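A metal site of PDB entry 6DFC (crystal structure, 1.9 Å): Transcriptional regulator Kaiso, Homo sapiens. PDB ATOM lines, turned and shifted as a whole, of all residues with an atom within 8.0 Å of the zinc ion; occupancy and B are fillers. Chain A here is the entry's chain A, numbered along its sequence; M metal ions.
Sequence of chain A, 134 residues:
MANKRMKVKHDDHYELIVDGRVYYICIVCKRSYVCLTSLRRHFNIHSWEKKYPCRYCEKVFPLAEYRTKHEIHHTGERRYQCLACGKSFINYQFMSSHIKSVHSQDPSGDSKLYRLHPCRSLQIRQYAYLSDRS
SG of Cys 85 lies close to N of Lys 87 (3.6 Å).
N of Ala 84 sits close to SG of Cys 82 (3.4 Å).
The backbone NH (N) of Cys 82 lies within hydrogen-bond range of the backbone carbonyl oxygen (O) of Lys 87 (2.8 Å).
NE2 of His 98 is bound to the zinc ion (2.0 Å).
The zinc ion is bound by NE2 of His 103, at 2.1 Å.
The zinc ion is bound by SG of Cys 85, at 2.3 Å.
SG of Cys 82 binds the zinc ion (2.3 Å).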
ATOM      1  N   GLN A  81     -25.805  23.786  16.788  1.00  0.00           N
ATOM      2  CA  GLN A  81     -24.533  24.068  16.129  1.00  0.00           C
ATOM      3  C   GLN A  81     -24.743  24.568  14.717  1.00  0.00           C
ATOM      4  O   GLN A  81     -25.413  23.907  13.914  1.00  0.00           O
ATOM      5  CB  GLN A  81     -23.637  22.833  16.092  1.00  0.00           C
ATOM      6  CG  GLN A  81     -22.211  23.124  15.491  1.00  0.00           C
ATOM      7  CD  GLN A  81     -21.248  21.978  15.661  1.00  0.00           C
ATOM      8  OE1 GLN A  81     -21.669  20.815  15.699  1.00  0.00           O
ATOM      9  NE2 GLN A  81     -19.922  22.271  15.711  1.00  0.00           N
ATOM     10  N   CYS A  82     -24.160  25.718  14.424  1.00  0.00           N
ATOM     11  CA  CYS A  82     -24.134  26.236  13.061  1.00  0.00           C
ATOM     12  C   CYS A  82     -23.303  25.345  12.137  1.00  0.00           C
ATOM     13  O   CYS A  82     -22.112  25.095  12.381  1.00  0.00           O
ATOM     14  CB  CYS A  82     -23.600  27.665  13.055  1.00  0.00           C
ATOM     15  SG  CYS A  82     -23.338  28.341  11.374  1.00  0.00           S
ATOM     16  N   LEU A  83     -23.910  24.857  11.073  1.00  0.00           N
ATOM     17  CA  LEU A  83     -23.197  23.945  10.188  1.00  0.00           C
ATOM     18  C   LEU A  83     -22.285  24.697   9.237  1.00  0.00           C
ATOM     19  O   LEU A  83     -21.409  24.107   8.645  1.00  0.00           O
ATOM     20  CB  LEU A  83     -24.168  23.080   9.405  1.00  0.00           C
ATOM     21  CG  LEU A  83     -24.981  22.113  10.271  1.00  0.00           C
ATOM     22  CD1 LEU A  83     -25.941  21.326   9.425  1.00  0.00           C
ATOM     23  CD2 LEU A  83     -24.065  21.183  11.044  1.00  0.00           C
ATOM     24  N   ALA A  84     -22.494  25.999   9.105  1.00  0.00           N
ATOM     25  CA  ALA A  84     -21.656  26.797   8.228  1.00  0.00           C
ATOM     26  C   ALA A  84     -20.263  27.030   8.809  1.00  0.00           C
ATOM     27  O   ALA A  84     -19.276  26.963   8.073  1.00  0.00           O
ATOM     28  CB  ALA A  84     -22.347  28.139   7.925  1.00  0.00           C
ATOM     29  N   CYS A  85     -20.160  27.281  10.116  1.00  0.00           N
ATOM     30  CA  CYS A  85     -18.878  27.629  10.733  1.00  0.00           C
ATOM     31  C   CYS A  85     -18.518  26.835  12.000  1.00  0.00           C
ATOM     32  O   CYS A  85     -17.425  27.006  12.546  1.00  0.00           O
ATOM     33  CB  CYS A  85     -18.862  29.123  11.070  1.00  0.00           C
ATOM     34  SG  CYS A  85     -19.875  29.568  12.527  1.00  0.00           S
ATOM     35  N   GLY A  86     -19.428  25.991  12.474  1.00  0.00           N
ATOM     36  CA  GLY A  86     -19.214  25.146  13.639  1.00  0.00           C
ATOM     37  C   GLY A  86     -19.494  25.720  15.023  1.00  0.00           C
ATOM     38  O   GLY A  86     -19.443  24.988  16.032  1.00  0.00           O
ATOM     39  N   LYS A  87     -19.783  27.026  15.091  1.00  0.00           N
ATOM     40  CA  LYS A  87     -20.080  27.644  16.396  1.00  0.00           C
ATOM     41  C   LYS A  87     -21.350  27.053  16.955  1.00  0.00           C
ATOM     42  O   LYS A  87     -22.265  26.719  16.193  1.00  0.00           O
ATOM     43  CB  LYS A  87     -20.227  29.151  16.285  1.00  0.00           C
ATOM     44  CG  LYS A  87     -18.940  29.932  15.988  1.00  0.00           C
ATOM     45  CD  LYS A  87     -19.090  31.359  16.493  1.00  0.00           C
ATOM     46  CE  LYS A  87     -18.016  32.287  15.951  1.00  0.00           C
ATOM     47  NZ  LYS A  87     -18.305  33.697  16.374  1.00  0.00           N
ATOM     48  N   SER A  88     -21.399  26.928  18.277  1.00  0.00           N
ATOM     49  CA  SER A  88     -22.520  26.294  18.973  1.00  0.00           C
ATOM     50  C   SER A  88     -23.206  27.272  19.905  1.00  0.00           C
ATOM     51  O   SER A  88     -22.578  28.202  20.403  1.00  0.00           O
ATOM     52  CB  SER A  88     -22.015  25.061  19.739  1.00  0.00           C
ATOM     53  OG  SER A  88     -21.407  24.165  18.829  1.00  0.00           O
ATOM     54  N   PHE A  89     -24.495  27.050  20.154  1.00  0.00           N
ATOM     55  CA  PHE A  89     -25.320  28.020  20.860  1.00  0.00           C
ATOM     56  C   PHE A  89     -26.209  27.273  21.820  1.00  0.00           C
ATOM     57  O   PHE A  89     -26.512  26.097  21.589  1.00  0.00           O
ATOM     58  CB  PHE A  89     -26.160  28.870  19.866  1.00  0.00           C
ATOM     59  CG  PHE A  89     -25.286  29.540  18.812  1.00  0.00           C
ATOM     60  CD1 PHE A  89     -24.706  30.775  19.068  1.00  0.00           C
ATOM     61  CD2 PHE A  89     -24.963  28.894  17.632  1.00  0.00           C
ATOM     62  CE1 PHE A  89     -23.851  31.369  18.152  1.00  0.00           C
ATOM     63  CE2 PHE A  89     -24.121  29.483  16.705  1.00  0.00           C
ATOM     64  CZ  PHE A  89     -23.567  30.728  16.978  1.00  0.00           C
ATOM     65  N   MET A  95     -28.824  30.641  17.924  1.00  0.00           N
ATOM     66  CA  MET A  95     -28.409  29.995  16.680  1.00  0.00           C
ATOM     67  C   MET A  95     -28.961  30.780  15.496  1.00  0.00           C
ATOM     68  O   MET A  95     -28.229  31.169  14.567  1.00  0.00           O
ATOM     69  CB  MET A  95     -28.890  28.532  16.660  1.00  0.00           C
ATOM     70  CG  MET A  95     -28.709  27.773  15.328  1.00  0.00           C
ATOM     71  SD  MET A  95     -29.939  28.129  14.050  1.00  0.00           S
ATOM     72  CE  MET A  95     -31.471  27.708  14.931  1.00  0.00           C
ATOM     73  N   HIS A  98     -27.456  34.232  14.890  1.00  0.00           N
ATOM     74  CA  HIS A  98     -26.119  34.055  14.331  1.00  0.00           C
ATOM     75  C   HIS A  98     -26.154  33.768  12.837  1.00  0.00           C
ATOM     76  O   HIS A  98     -25.475  34.425  12.043  1.00  0.00           O
ATOM     77  CB  HIS A  98     -25.405  32.914  15.046  1.00  0.00           C
ATOM     78  CG  HIS A  98     -24.191  32.429  14.307  1.00  0.00           C
ATOM     79  ND1 HIS A  98     -23.000  33.113  14.320  1.00  0.00           N
ATOM     80  CD2 HIS A  98     -24.018  31.362  13.506  1.00  0.00           C
ATOM     81  CE1 HIS A  98     -22.116  32.457  13.582  1.00  0.00           C
ATOM     82  NE2 HIS A  98     -22.703  31.396  13.073  1.00  0.00           N
ATOM     83  N   ILE A  99     -26.966  32.791  12.442  1.00  0.00           N
ATOM     84  CA  ILE A  99     -26.990  32.403  11.043  1.00  0.00           C
ATOM     85  C   ILE A  99     -27.534  33.530  10.188  1.00  0.00           C
ATOM     86  O   ILE A  99     -27.008  33.786   9.109  1.00  0.00           O
ATOM     87  CB  ILE A  99     -27.810  31.118  10.864  1.00  0.00           C
ATOM     88  CG1 ILE A  99     -27.079  29.986  11.612  1.00  0.00           C
ATOM     89  CG2 ILE A  99     -27.951  30.782   9.390  1.00  0.00           C
ATOM     90  CD1 ILE A  99     -27.590  28.608  11.337  1.00  0.00           C
ATOM     91  N   LYS A 100     -28.541  34.254  10.677  1.00  0.00           N
ATOM     92  CA  LYS A 100     -29.051  35.372   9.910  1.00  0.00           C
ATOM     93  C   LYS A 100     -28.045  36.519   9.775  1.00  0.00           C
ATOM     94  O   LYS A 100     -27.878  37.073   8.689  1.00  0.00           O
ATOM     95  CB  LYS A 100     -30.349  35.888  10.552  1.00  0.00           C
ATOM     96  CG  LYS A 100     -31.504  34.929  10.361  1.00  0.00           C
ATOM     97  CD  LYS A 100     -32.772  35.432  11.069  1.00  0.00           C
ATOM     98  CE  LYS A 100     -33.981  34.597  10.690  1.00  0.00           C
ATOM     99  NZ  LYS A 100     -35.223  35.010  11.443  1.00  0.00           N
ATOM    100  N   VAL A 102     -24.565  36.542  10.545  1.00  0.00           N
ATOM    101  CA  VAL A 102     -23.226  36.192  10.082  1.00  0.00           C
ATOM    102  C   VAL A 102     -23.249  35.583   8.682  1.00  0.00           C
ATOM    103  O   VAL A 102     -22.445  35.958   7.834  1.00  0.00           O
ATOM    104  CB  VAL A 102     -22.525  35.232  11.072  1.00  0.00           C
ATOM    105  CG1 VAL A 102     -21.207  34.764  10.514  1.00  0.00           C
ATOM    106  CG2 VAL A 102     -22.305  35.939  12.403  1.00  0.00           C
ATOM    107  N   HIS A 103     -24.184  34.678   8.418  1.00  0.00           N
ATOM    108  CA  HIS A 103     -24.214  33.953   7.142  1.00  0.00           C
ATOM    109  C   HIS A 103     -25.307  34.421   6.173  1.00  0.00           C
ATOM    110  O   HIS A 103     -25.392  33.927   5.055  1.00  0.00           O
ATOM    111  CB  HIS A 103     -24.356  32.467   7.410  1.00  0.00           C
ATOM    112  CG  HIS A 103     -23.270  31.911   8.281  1.00  0.00           C
ATOM    113  ND1 HIS A 103     -21.938  31.973   7.929  1.00  0.00           N
ATOM    114  CD2 HIS A 103     -23.302  31.354   9.518  1.00  0.00           C
ATOM    115  CE1 HIS A 103     -21.202  31.445   8.892  1.00  0.00           C
ATOM    116  NE2 HIS A 103     -21.999  31.057   9.861  1.00  0.00           N
ATOM    117  N   LEU A 113     -29.357  24.246   8.179  1.00  0.00           N
ATOM    118  CA  LEU A 113     -28.208  25.117   8.345  1.00  0.00           C
ATOM    119  C   LEU A 113     -27.635  24.904   9.734  1.00  0.00           C
ATOM    120  O   LEU A 113     -26.601  25.460  10.095  1.00  0.00           O
ATOM    121  CB  LEU A 113     -28.625  26.570   8.188  1.00  0.00           C
ATOM    122  CG  LEU A 113     -29.245  26.934   6.817  1.00  0.00           C
ATOM    123  CD1 LEU A 113     -29.636  28.393   6.816  1.00  0.00           C
ATOM    124  CD2 LEU A 113     -28.260  26.646   5.692  1.00  0.00           C
HETATM  125 ZN    ZN M   1     -21.923  30.115  11.717  1.00  0.00          ZN
